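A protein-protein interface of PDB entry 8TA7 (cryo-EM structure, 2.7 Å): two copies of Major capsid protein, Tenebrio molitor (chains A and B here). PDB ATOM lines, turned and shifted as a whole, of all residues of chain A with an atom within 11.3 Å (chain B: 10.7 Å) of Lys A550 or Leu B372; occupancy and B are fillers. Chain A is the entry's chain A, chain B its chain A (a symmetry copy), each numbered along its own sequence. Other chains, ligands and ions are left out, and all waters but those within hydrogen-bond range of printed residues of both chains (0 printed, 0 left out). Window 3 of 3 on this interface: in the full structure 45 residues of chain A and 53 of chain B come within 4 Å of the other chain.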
ATOM      1  N   HIS A 175      11.288  30.397   8.410  1.00  0.00           N
ATOM      2  CA  HIS A 175      11.223  31.786   8.835  1.00  0.00           C
ATOM      3  C   HIS A 175      12.551  32.454   8.507  1.00  0.00           C
ATOM      4  O   HIS A 175      13.545  32.263   9.215  1.00  0.00           O
ATOM      5  CB  HIS A 175      10.924  31.877  10.326  1.00  0.00           C
ATOM      6  CG  HIS A 175      10.726  33.277  10.816  1.00  0.00           C
ATOM      7  ND1 HIS A 175      10.885  33.630  12.139  1.00  0.00           N
ATOM      8  CD2 HIS A 175      10.383  34.411  10.163  1.00  0.00           C
ATOM      9  CE1 HIS A 175      10.656  34.923  12.277  1.00  0.00           C
ATOM     10  NE2 HIS A 175      10.347  35.421  11.093  1.00  0.00           N
ATOM     11  N   PHE A 411      25.395  32.924   8.662  1.00  0.00           N
ATOM     12  CA  PHE A 411      25.223  32.133   9.870  1.00  0.00           C
ATOM     13  C   PHE A 411      25.738  30.718   9.644  1.00  0.00           C
ATOM     14  O   PHE A 411      25.547  30.136   8.573  1.00  0.00           O
ATOM     15  CB  PHE A 411      23.750  32.083  10.279  1.00  0.00           C
ATOM     16  CG  PHE A 411      23.330  33.190  11.199  1.00  0.00           C
ATOM     17  CD1 PHE A 411      23.800  33.242  12.497  1.00  0.00           C
ATOM     18  CD2 PHE A 411      22.439  34.160  10.774  1.00  0.00           C
ATOM     19  CE1 PHE A 411      23.405  34.250  13.349  1.00  0.00           C
ATOM     20  CE2 PHE A 411      22.039  35.171  11.622  1.00  0.00           C
ATOM     21  CZ  PHE A 411      22.519  35.213  12.914  1.00  0.00           C
ATOM     22  N   ALA A 412      26.398  30.167  10.655  1.00  0.00           N
ATOM     23  CA  ALA A 412      26.854  28.794  10.562  1.00  0.00           C
ATOM     24  C   ALA A 412      25.658  27.844  10.587  1.00  0.00           C
ATOM     25  O   ALA A 412      24.690  28.066  11.322  1.00  0.00           O
ATOM     26  CB  ALA A 412      27.809  28.465  11.707  1.00  0.00           C
ATOM     27  N   PRO A 413      25.687  26.788   9.782  1.00  0.00           N
ATOM     28  CA  PRO A 413      24.632  25.774   9.853  1.00  0.00           C
ATOM     29  C   PRO A 413      24.870  24.818  11.011  1.00  0.00           C
ATOM     30  O   PRO A 413      25.926  24.804  11.645  1.00  0.00           O
ATOM     31  CB  PRO A 413      24.747  25.061   8.507  1.00  0.00           C
ATOM     32  CG  PRO A 413      26.187  25.181   8.164  1.00  0.00           C
ATOM     33  CD  PRO A 413      26.631  26.523   8.682  1.00  0.00           C
ATOM     34  N   VAL A 414      23.856  24.006  11.286  1.00  0.00           N
ATOM     35  CA  VAL A 414      24.022  22.889  12.210  1.00  0.00           C
ATOM     36  C   VAL A 414      24.859  21.842  11.485  1.00  0.00           C
ATOM     37  O   VAL A 414      24.457  21.367  10.414  1.00  0.00           O
ATOM     38  CB  VAL A 414      22.670  22.322  12.668  1.00  0.00           C
ATOM     39  CG1 VAL A 414      22.878  21.087  13.526  1.00  0.00           C
ATOM     40  CG2 VAL A 414      21.890  23.372  13.433  1.00  0.00           C
ATOM     41  N   PRO A 415      26.021  21.461  12.016  1.00  0.00           N
ATOM     42  CA  PRO A 415      26.899  20.531  11.286  1.00  0.00           C
ATOM     43  C   PRO A 415      26.273  19.147  11.216  1.00  0.00           C
ATOM     44  O   PRO A 415      25.888  18.572  12.236  1.00  0.00           O
ATOM     45  CB  PRO A 415      28.195  20.532  12.104  1.00  0.00           C
ATOM     46  CG  PRO A 415      27.927  21.288  13.345  1.00  0.00           C
ATOM     47  CD  PRO A 415      26.549  21.845  13.335  1.00  0.00           C
ATOM     48  N   LEU A 418      27.420  15.784  13.118  1.00  0.00           N
ATOM     49  CA  LEU A 418      26.916  15.468  14.446  1.00  0.00           C
ATOM     50  C   LEU A 418      25.651  14.627  14.401  1.00  0.00           C
ATOM     51  O   LEU A 418      25.221  14.119  15.442  1.00  0.00           O
ATOM     52  CB  LEU A 418      26.635  16.756  15.222  1.00  0.00           C
ATOM     53  CG  LEU A 418      27.797  17.730  15.408  1.00  0.00           C
ATOM     54  CD1 LEU A 418      27.324  18.968  16.142  1.00  0.00           C
ATOM     55  CD2 LEU A 418      28.938  17.064  16.153  1.00  0.00           C
ATOM     56  N   ILE A 419      25.047  14.477  13.225  1.00  0.00           N
ATOM     57  CA  ILE A 419      23.779  13.787  13.093  1.00  0.00           C
ATOM     58  C   ILE A 419      23.862  12.584  12.156  1.00  0.00           C
ATOM     59  O   ILE A 419      23.061  11.652  12.292  1.00  0.00           O
ATOM     60  CB  ILE A 419      22.689  14.773  12.621  1.00  0.00           C
ATOM     61  CG1 ILE A 419      22.729  16.055  13.451  1.00  0.00           C
ATOM     62  CG2 ILE A 419      21.321  14.164  12.752  1.00  0.00           C
ATOM     63  CD1 ILE A 419      21.807  17.136  12.940  1.00  0.00           C
ATOM     64  N   PRO A 545      18.102  33.222   8.895  1.00  0.00           N
ATOM     65  CA  PRO A 545      17.284  32.014   8.717  1.00  0.00           C
ATOM     66  C   PRO A 545      17.074  31.226  10.005  1.00  0.00           C
ATOM     67  O   PRO A 545      18.036  30.957  10.730  1.00  0.00           O
ATOM     68  CB  PRO A 545      18.096  31.210   7.699  1.00  0.00           C
ATOM     69  CG  PRO A 545      19.522  31.574   8.012  1.00  0.00           C
ATOM     70  CD  PRO A 545      19.527  32.961   8.627  1.00  0.00           C
ATOM     71  N   TYR A 546      15.836  30.848  10.310  1.00  0.00           N
ATOM     72  CA  TYR A 546      15.554  30.017  11.481  1.00  0.00           C
ATOM     73  C   TYR A 546      15.272  28.575  11.057  1.00  0.00           C
ATOM     74  O   TYR A 546      14.132  28.117  11.002  1.00  0.00           O
ATOM     75  CB  TYR A 546      14.401  30.611  12.278  1.00  0.00           C
ATOM     76  CG  TYR A 546      14.745  31.948  12.877  1.00  0.00           C
ATOM     77  CD1 TYR A 546      15.478  32.033  14.051  1.00  0.00           C
ATOM     78  CD2 TYR A 546      14.358  33.127  12.258  1.00  0.00           C
ATOM     79  CE1 TYR A 546      15.802  33.250  14.598  1.00  0.00           C
ATOM     80  CE2 TYR A 546      14.680  34.351  12.799  1.00  0.00           C
ATOM     81  CZ  TYR A 546      15.401  34.407  13.969  1.00  0.00           C
ATOM     82  OH  TYR A 546      15.725  35.624  14.516  1.00  0.00           O
ATOM     83  N   THR A 547      16.353  27.852  10.757  1.00  0.00           N
ATOM     84  CA  THR A 547      16.214  26.463  10.335  1.00  0.00           C
ATOM     85  C   THR A 547      15.966  25.514  11.501  1.00  0.00           C
ATOM     86  O   THR A 547      15.609  24.355  11.271  1.00  0.00           O
ATOM     87  CB  THR A 547      17.455  26.009   9.564  1.00  0.00           C
ATOM     88  OG1 THR A 547      18.620  26.199  10.374  1.00  0.00           O
ATOM     89  CG2 THR A 547      17.598  26.800   8.279  1.00  0.00           C
ATOM     90  N   TYR A 548      16.146  25.969  12.737  1.00  0.00           N
ATOM     91  CA  TYR A 548      15.964  25.131  13.911  1.00  0.00           C
ATOM     92  C   TYR A 548      15.174  25.889  14.969  1.00  0.00           C
ATOM     93  O   TYR A 548      14.981  27.104  14.881  1.00  0.00           O
ATOM     94  CB  TYR A 548      17.307  24.661  14.480  1.00  0.00           C
ATOM     95  CG  TYR A 548      17.830  23.404  13.825  1.00  0.00           C
ATOM     96  CD1 TYR A 548      18.356  23.434  12.540  1.00  0.00           C
ATOM     97  CD2 TYR A 548      17.795  22.186  14.487  1.00  0.00           C
ATOM     98  CE1 TYR A 548      18.828  22.289  11.935  1.00  0.00           C
ATOM     99  CE2 TYR A 548      18.267  21.037  13.891  1.00  0.00           C
ATOM    100  CZ  TYR A 548      18.782  21.093  12.616  1.00  0.00           C
ATOM    101  OH  TYR A 548      19.255  19.949  12.019  1.00  0.00           O
ATOM    102  N   ILE A 549      14.721  25.148  15.980  1.00  0.00           N
ATOM    103  CA  ILE A 549      13.799  25.709  16.960  1.00  0.00           C
ATOM    104  C   ILE A 549      14.531  26.450  18.073  1.00  0.00           C
ATOM    105  O   ILE A 549      14.088  27.521  18.501  1.00  0.00           O
ATOM    106  CB  ILE A 549      12.896  24.598  17.523  1.00  0.00           C
ATOM    107  CG1 ILE A 549      11.929  24.109  16.447  1.00  0.00           C
ATOM    108  CG2 ILE A 549      12.134  25.083  18.743  1.00  0.00           C
ATOM    109  CD1 ILE A 549      11.178  22.863  16.830  1.00  0.00           C
ATOM    110  N   LYS A 550      15.649  25.918  18.556  1.00  0.00           N
ATOM    111  CA  LYS A 550      16.327  26.472  19.717  1.00  0.00           C
ATOM    112  C   LYS A 550      17.685  27.032  19.318  1.00  0.00           C
ATOM    113  O   LYS A 550      18.128  26.902  18.176  1.00  0.00           O
ATOM    114  CB  LYS A 550      16.500  25.416  20.816  1.00  0.00           C
ATOM    115  CG  LYS A 550      15.251  24.606  21.082  1.00  0.00           C
ATOM    116  CD  LYS A 550      15.408  23.730  22.306  1.00  0.00           C
ATOM    117  CE  LYS A 550      15.257  24.539  23.577  1.00  0.00           C
ATOM    118  NZ  LYS A 550      13.840  24.911  23.812  1.00  0.00           N
ATOM    119  N   GLY A 551      18.335  27.671  20.283  1.00  0.00           N
ATOM    120  CA  GLY A 551      19.690  28.193  20.104  1.00  0.00           C
ATOM    121  C   GLY A 551      19.834  29.543  19.442  1.00  0.00           C
ATOM    122  O   GLY A 551      20.341  30.483  20.057  1.00  0.00           O
ATOM    123  N   GLY A 552      19.398  29.663  18.197  1.00  0.00           N
ATOM    124  CA  GLY A 552      19.551  30.898  17.455  1.00  0.00           C
ATOM    125  C   GLY A 552      19.369  30.634  15.973  1.00  0.00           C
ATOM    126  O   GLY A 552      18.769  29.638  15.577  1.00  0.00           O
ATOM    127  N   CYS A 553      19.898  31.549  15.168  1.00  0.00           N
ATOM    128  CA  CYS A 553      19.852  31.363  13.725  1.00  0.00           C
ATOM    129  C   CYS A 553      20.886  30.346  13.274  1.00  0.00           C
ATOM    130  O   CYS A 553      22.039  30.363  13.711  1.00  0.00           O
ATOM    131  CB  CYS A 553      20.079  32.684  12.999  1.00  0.00           C
ATOM    132  SG  CYS A 553      18.676  33.785  13.012  1.00  0.00           S
ATOM    133  N   TYR A 554      20.455  29.453  12.392  1.00  0.00           N
ATOM    134  CA  TYR A 554      21.327  28.513  11.712  1.00  0.00           C
ATOM    135  C   TYR A 554      20.946  28.515  10.244  1.00  0.00           C
ATOM    136  O   TYR A 554      19.760  28.509   9.908  1.00  0.00           O
ATOM    137  CB  TYR A 554      21.202  27.102  12.294  1.00  0.00           C
ATOM    138  CG  TYR A 554      21.684  26.980  13.719  1.00  0.00           C
ATOM    139  CD1 TYR A 554      23.022  26.754  14.002  1.00  0.00           C
ATOM    140  CD2 TYR A 554      20.799  27.097  14.780  1.00  0.00           C
ATOM    141  CE1 TYR A 554      23.466  26.643  15.302  1.00  0.00           C
ATOM    142  CE2 TYR A 554      21.235  26.990  16.083  1.00  0.00           C
ATOM    143  CZ  TYR A 554      22.568  26.762  16.339  1.00  0.00           C
ATOM    144  OH  TYR A 554      23.004  26.652  17.639  1.00  0.00           O
ATOM    145  N   SER A 555      21.946  28.541   9.373  1.00  0.00           N
ATOM    146  CA  SER A 555      21.665  28.526   7.951  1.00  0.00           C
ATOM    147  C   SER A 555      21.496  27.095   7.455  1.00  0.00           C
ATOM    148  O   SER A 555      21.832  26.127   8.141  1.00  0.00           O
ATOM    149  CB  SER A 555      22.787  29.212   7.172  1.00  0.00           C
ATOM    150  OG  SER A 555      22.905  30.574   7.534  1.00  0.00           O
ATOM    151  N   ILE B 198      10.326  10.704  20.796  1.00  0.00           N
ATOM    152  CA  ILE B 198      11.763  10.847  20.604  1.00  0.00           C
ATOM    153  C   ILE B 198      12.435   9.540  21.003  1.00  0.00           C
ATOM    154  O   ILE B 198      12.247   9.048  22.120  1.00  0.00           O
ATOM    155  CB  ILE B 198      12.326  12.027  21.406  1.00  0.00           C
ATOM    156  CG1 ILE B 198      11.752  13.347  20.895  1.00  0.00           C
ATOM    157  CG2 ILE B 198      13.833  12.059  21.305  1.00  0.00           C
ATOM    158  CD1 ILE B 198      12.062  14.516  21.788  1.00  0.00           C
ATOM    159  N   TRP B 211      19.201  11.858  18.470  1.00  0.00           N
ATOM    160  CA  TRP B 211      17.809  11.750  18.874  1.00  0.00           C
ATOM    161  C   TRP B 211      16.950  11.601  17.629  1.00  0.00           C
ATOM    162  O   TRP B 211      17.116  12.352  16.662  1.00  0.00           O
ATOM    163  CB  TRP B 211      17.371  12.989  19.654  1.00  0.00           C
ATOM    164  CG  TRP B 211      18.014  13.151  20.987  1.00  0.00           C
ATOM    165  CD1 TRP B 211      18.906  14.111  21.352  1.00  0.00           C
ATOM    166  CD2 TRP B 211      17.797  12.344  22.148  1.00  0.00           C
ATOM    167  NE1 TRP B 211      19.268  13.949  22.664  1.00  0.00           N
ATOM    168  CE2 TRP B 211      18.597  12.870  23.176  1.00  0.00           C
ATOM    169  CE3 TRP B 211      17.006  11.224  22.416  1.00  0.00           C
ATOM    170  CZ2 TRP B 211      18.629  12.317  24.449  1.00  0.00           C
ATOM    171  CZ3 TRP B 211      17.038  10.680  23.677  1.00  0.00           C
ATOM    172  CH2 TRP B 211      17.843  11.224  24.680  1.00  0.00           C
ATOM    173  N   THR B 360      18.145  14.712  15.263  1.00  0.00           N
ATOM    174  CA  THR B 360      18.902  15.837  15.785  1.00  0.00           C
ATOM    175  C   THR B 360      20.073  15.281  16.579  1.00  0.00           C
ATOM    176  O   THR B 360      20.096  14.102  16.935  1.00  0.00           O
ATOM    177  CB  THR B 360      18.030  16.764  16.642  1.00  0.00           C
ATOM    178  OG1 THR B 360      18.662  18.042  16.766  1.00  0.00           O
ATOM    179  CG2 THR B 360      17.807  16.175  18.022  1.00  0.00           C
ATOM    180  N   ASN B 361      21.066  16.126  16.828  1.00  0.00           N
ATOM    181  CA  ASN B 361      22.252  15.663  17.530  1.00  0.00           C
ATOM    182  C   ASN B 361      21.942  15.380  18.996  1.00  0.00           C
ATOM    183  O   ASN B 361      21.040  15.973  19.591  1.00  0.00           O
ATOM    184  CB  ASN B 361      23.381  16.687  17.413  1.00  0.00           C
ATOM    185  CG  ASN B 361      23.023  18.022  18.028  1.00  0.00           C
ATOM    186  OD1 ASN B 361      22.219  18.774  17.480  1.00  0.00           O
ATOM    187  ND2 ASN B 361      23.623  18.325  19.171  1.00  0.00           N
ATOM    188  N   ASP B 362      22.698  14.451  19.572  1.00  0.00           N
ATOM    189  CA  ASP B 362      22.574  14.082  20.979  1.00  0.00           C
ATOM    190  C   ASP B 362      23.827  14.580  21.690  1.00  0.00           C
ATOM    191  O   ASP B 362      24.898  13.977  21.584  1.00  0.00           O
ATOM    192  CB  ASP B 362      22.395  12.574  21.128  1.00  0.00           C
ATOM    193  CG  ASP B 362      22.183  12.143  22.564  1.00  0.00           C
ATOM    194  OD1 ASP B 362      22.111  13.014  23.454  1.00  0.00           O
ATOM    195  OD2 ASP B 362      22.087  10.923  22.806  1.00  0.00           O
ATOM    196  N   ALA B 363      23.686  15.682  22.426  1.00  0.00           N
ATOM    197  CA  ALA B 363      24.831  16.337  23.040  1.00  0.00           C
ATOM    198  C   ALA B 363      25.030  15.963  24.502  1.00  0.00           C
ATOM    199  O   ALA B 363      25.747  16.679  25.208  1.00  0.00           O
ATOM    200  CB  ALA B 363      24.693  17.855  22.913  1.00  0.00           C
ATOM    201  N   ARG B 364      24.413  14.879  24.979  1.00  0.00           N
ATOM    202  CA  ARG B 364      24.601  14.484  26.371  1.00  0.00           C
ATOM    203  C   ARG B 364      26.058  14.145  26.659  1.00  0.00           C
ATOM    204  O   ARG B 364      26.609  14.559  27.685  1.00  0.00           O
ATOM    205  CB  ARG B 364      23.703  13.296  26.713  1.00  0.00           C
ATOM    206  CG  ARG B 364      22.221  13.616  26.743  1.00  0.00           C
ATOM    207  CD  ARG B 364      21.418  12.381  27.101  1.00  0.00           C
ATOM    208  NE  ARG B 364      21.480  11.365  26.059  1.00  0.00           N
ATOM    209  CZ  ARG B 364      20.734  10.269  26.038  1.00  0.00           C
ATOM    210  NH1 ARG B 364      19.857  10.013  26.996  1.00  0.00           N
ATOM    211  NH2 ARG B 364      20.870   9.410  25.034  1.00  0.00           N
ATOM    212  N   ALA B 365      26.696  13.389  25.768  1.00  0.00           N
ATOM    213  CA  ALA B 365      28.094  13.018  25.929  1.00  0.00           C
ATOM    214  C   ALA B 365      29.043  13.876  25.106  1.00  0.00           C
ATOM    215  O   ALA B 365      30.248  13.610  25.105  1.00  0.00           O
ATOM    216  CB  ALA B 365      28.296  11.544  25.563  1.00  0.00           C
ATOM    217  N   THR B 366      28.536  14.887  24.404  1.00  0.00           N
ATOM    218  CA  THR B 366      29.394  15.735  23.589  1.00  0.00           C
ATOM    219  C   THR B 366      30.266  16.614  24.477  1.00  0.00           C
ATOM    220  O   THR B 366      29.769  17.288  25.384  1.00  0.00           O
ATOM    221  CB  THR B 366      28.550  16.600  22.651  1.00  0.00           C
ATOM    222  OG1 THR B 366      27.949  15.771  21.649  1.00  0.00           O
ATOM    223  CG2 THR B 366      29.412  17.657  21.977  1.00  0.00           C
ATOM    224  N   THR B 367      31.567  16.608  24.210  1.00  0.00           N
ATOM    225  CA  THR B 367      32.531  17.392  24.967  1.00  0.00           C
ATOM    226  C   THR B 367      33.057  18.534  24.106  1.00  0.00           C
ATOM    227  O   THR B 367      33.463  18.324  22.958  1.00  0.00           O
ATOM    228  CB  THR B 367      33.692  16.517  25.444  1.00  0.00           C
ATOM    229  OG1 THR B 367      33.196  15.505  26.329  1.00  0.00           O
ATOM    230  CG2 THR B 367      34.729  17.352  26.175  1.00  0.00           C
ATOM    231  N   GLY B 368      33.042  19.738  24.661  1.00  0.00           N
ATOM    232  CA  GLY B 368      33.523  20.906  23.943  1.00  0.00           C
ATOM    233  C   GLY B 368      32.381  21.822  23.550  1.00  0.00           C
ATOM    234  O   GLY B 368      31.603  22.254  24.402  1.00  0.00           O
ATOM    235  N   THR B 369      32.285  22.124  22.258  1.00  0.00           N
ATOM    236  CA  THR B 369      31.244  23.012  21.748  1.00  0.00           C
ATOM    237  C   THR B 369      29.993  22.195  21.462  1.00  0.00           C
ATOM    238  O   THR B 369      29.975  21.350  20.565  1.00  0.00           O
ATOM    239  CB  THR B 369      31.724  23.733  20.494  1.00  0.00           C
ATOM    240  OG1 THR B 369      32.886  24.512  20.802  1.00  0.00           O
ATOM    241  CG2 THR B 369      30.635  24.650  19.962  1.00  0.00           C
ATOM    242  N   LYS B 370      28.936  22.444  22.228  1.00  0.00           N
ATOM    243  CA  LYS B 370      27.691  21.708  22.063  1.00  0.00           C
ATOM    244  C   LYS B 370      26.694  22.517  21.246  1.00  0.00           C
ATOM    245  O   LYS B 370      26.475  23.703  21.501  1.00  0.00           O
ATOM    246  CB  LYS B 370      27.090  21.362  23.425  1.00  0.00           C
ATOM    247  CG  LYS B 370      27.954  20.441  24.265  1.00  0.00           C
ATOM    248  CD  LYS B 370      27.124  19.668  25.269  1.00  0.00           C
ATOM    249  CE  LYS B 370      26.676  20.560  26.412  1.00  0.00           C
ATOM    250  NZ  LYS B 370      26.598  19.814  27.699  1.00  0.00           N
ATOM    251  N   ILE B 371      26.094  21.866  20.256  1.00  0.00           N
ATOM    252  CA  ILE B 371      25.015  22.449  19.470  1.00  0.00           C
ATOM    253  C   ILE B 371      23.703  22.049  20.126  1.00  0.00           C
ATOM    254  O   ILE B 371      23.380  20.858  20.211  1.00  0.00           O
ATOM    255  CB  ILE B 371      25.068  21.986  18.005  1.00  0.00           C
ATOM    256  CG1 ILE B 371      26.358  22.464  17.337  1.00  0.00           C
ATOM    257  CG2 ILE B 371      23.857  22.495  17.240  1.00  0.00           C
ATOM    258  CD1 ILE B 371      26.459  23.967  17.213  1.00  0.00           C
ATOM    259  N   LEU B 372      22.950  23.039  20.599  1.00  0.00           N
ATOM    260  CA  LEU B 372      21.720  22.800  21.340  1.00  0.00           C
ATOM    261  C   LEU B 372      20.515  23.405  20.630  1.00  0.00           C
ATOM    262  O   LEU B 372      19.679  24.060  21.254  1.00  0.00           O
ATOM    263  CB  LEU B 372      21.835  23.337  22.765  1.00  0.00           C
ATOM    264  CG  LEU B 372      23.007  22.796  23.583  1.00  0.00           C
ATOM    265  CD1 LEU B 372      22.934  23.293  25.012  1.00  0.00           C
ATOM    266  CD2 LEU B 372      23.042  21.279  23.539  1.00  0.00           C
ATOM    267  N   ALA B 373      20.420  23.191  19.319  1.00  0.00           N
ATOM    268  CA  ALA B 373      19.342  23.763  18.526  1.00  0.00           C
ATOM    269  C   ALA B 373      18.046  22.969  18.612  1.00  0.00           C
ATOM    270  O   ALA B 373      17.018  23.449  18.124  1.00  0.00           O
ATOM    271  CB  ALA B 373      19.777  23.873  17.066  1.00  0.00           C
ATOM    272  N   GLY B 374      18.062  21.784  19.216  1.00  0.00           N
ATOM    273  CA  GLY B 374      16.848  20.993  19.261  1.00  0.00           C
ATOM    274  C   GLY B 374      16.498  20.417  17.900  1.00  0.00           C
ATOM    275  O   GLY B 374      17.362  20.100  17.080  1.00  0.00           O
ATOM    276  N   PHE B 375      15.203  20.276  17.662  1.00  0.00           N
ATOM    277  CA  PHE B 375      14.712  19.738  16.405  1.00  0.00           C
ATOM    278  C   PHE B 375      14.384  20.865  15.428  1.00  0.00           C
ATOM    279  O   PHE B 375      14.158  22.003  15.838  1.00  0.00           O
ATOM    280  CB  PHE B 375      13.468  18.891  16.642  1.00  0.00           C
ATOM    281  CG  PHE B 375      13.764  17.479  17.039  1.00  0.00           C
ATOM    282  CD1 PHE B 375      13.483  17.036  18.319  1.00  0.00           C
ATOM    283  CD2 PHE B 375      14.325  16.595  16.136  1.00  0.00           C
ATOM    284  CE1 PHE B 375      13.755  15.740  18.687  1.00  0.00           C
ATOM    285  CE2 PHE B 375      14.599  15.296  16.502  1.00  0.00           C
ATOM    286  CZ  PHE B 375      14.314  14.869  17.779  1.00  0.00           C
ATOM    287  N   PRO B 376      14.379  20.576  14.126  1.00  0.00           N
ATOM    288  CA  PRO B 376      13.842  21.542  13.173  1.00  0.00           C
ATOM    289  C   PRO B 376      12.328  21.448  13.120  1.00  0.00           C
ATOM    290  O   PRO B 376      11.749  20.374  13.358  1.00  0.00           O
ATOM    291  CB  PRO B 376      14.479  21.114  11.840  1.00  0.00           C
ATOM    292  CG  PRO B 376      14.708  19.661  12.004  1.00  0.00           C
ATOM    293  CD  PRO B 376      15.048  19.449  13.453  1.00  0.00           C
ATOM    294  N   PRO B 377      11.639  22.548  12.816  1.00  0.00           N
ATOM    295  CA  PRO B 377      10.166  22.530  12.744  1.00  0.00           C
ATOM    296  C   PRO B 377       9.656  21.884  11.459  1.00  0.00           C
ATOM    297  O   PRO B 377       9.201  22.555  10.530  1.00  0.00           O
ATOM    298  CB  PRO B 377       9.819  24.020  12.836  1.00  0.00           C
ATOM    299  CG  PRO B 377      10.969  24.694  12.175  1.00  0.00           C
ATOM    300  CD  PRO B 377      12.189  23.887  12.533  1.00  0.00           C
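The backbone NH (N) of Ile A549 lies close to the backbone carbonyl oxygen (O) of Phe B375 (3.2 Å).
The backbone NH of Lys A550 sits at hydrogen-bond distance from the backbone carbonyl oxygen of Ala B373 (2.9 Å).
The backbone carbonyl oxygen of Pro A545 is in hydrogen-bond range of the backbone NH of Tyr A554, at 3.3 Å.
The side-chain hydroxyl (OG1) of Thr A547 sits at hydrogen-bond distance from the backbone carbonyl oxygen (O) of Tyr A554, 2.6 Å away.
OG1 of Thr B360 lies within hydrogen-bond range of O of Gly B374, at 2.5 Å.
ND2 of Asn B361 lies within hydrogen-bond range of O of Ile B371 (2.7 Å).
Among the printed residues, merely in contact across the chains: Tyr A548 with Gly B374 (3.4 Å), Thr A547 with Pro B376 (3.5 Å), Lys A550 with Leu B372 (3.5 Å), Ile A549 with Ala B373 (3.6 Å), Tyr A554 with Ala B373 (3.6 Å), Tyr A548 with Pro B376 (3.6 Å), Tyr A548 with Ala B373 (3.7 Å), Thr A547 with Pro B377 (3.7 Å), Leu A418 with Asn B361 (3.7 Å), Ile A419 with Asn B361 (3.8 Å), Tyr A548 with Phe B375 (3.8 Å), Leu A418 with Ile B371 (3.8 Å), Ile A549 with Pro B377 (3.9 Å) and Gly A551 with Leu B372 (3.97 Å).
Printed residues of chain B within 4 Å of Leu A418: Asn B361 and Ile B371.
Printed residues of chain B within 4 Å of Ile A419: Asn B361 (3.8 Å).
Ile A549 touches just these residues of chain B: Ala B373 (3.6 Å), Phe B375 (3.1 Å) and Pro B377 (3.9 Å).
Of chain B, only Leu B372 (3.5 Å) and Ala B373 (2.9 Å) come within 4 Å of Lys A550.
Of the printed residues of chain B, Tyr A554 touches Ala B373.
Thr B360 touches none of the printed residues of chain A.
Of the printed residues of chain A, Asn B361 touches Leu A418 (3.7 Å) and Ile A419 (3.8 Å).
No residue of chain A comes within 4 Å of Ala B363.
Arg B364 touches none of the printed residues of chain A.
No residue of chain A comes within 4 Å of Lys B370.
Of the printed residues of chain A, Leu B372 touches Lys A550 and Gly A551.
Gly B374 touches just one residue of chain A: Tyr A548.
Of the printed residues of chain A, Phe B375 touches Tyr A548 (3.8 Å) and Ile A549 (3.1 Å).
Of the 19 printed residues of chain A, 8 touch a printed residue of chain B.
Hydrophobic or aromatic side chains of chain B within 4 Å of the printed part of chain A: Ile B371, Ala B373, Pro B376 and Pro B377.
No position is printed for both chains.
Of the 16 pairs that touch across the chains among the printed residues, none has its exchanged pair printed and touching as well.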
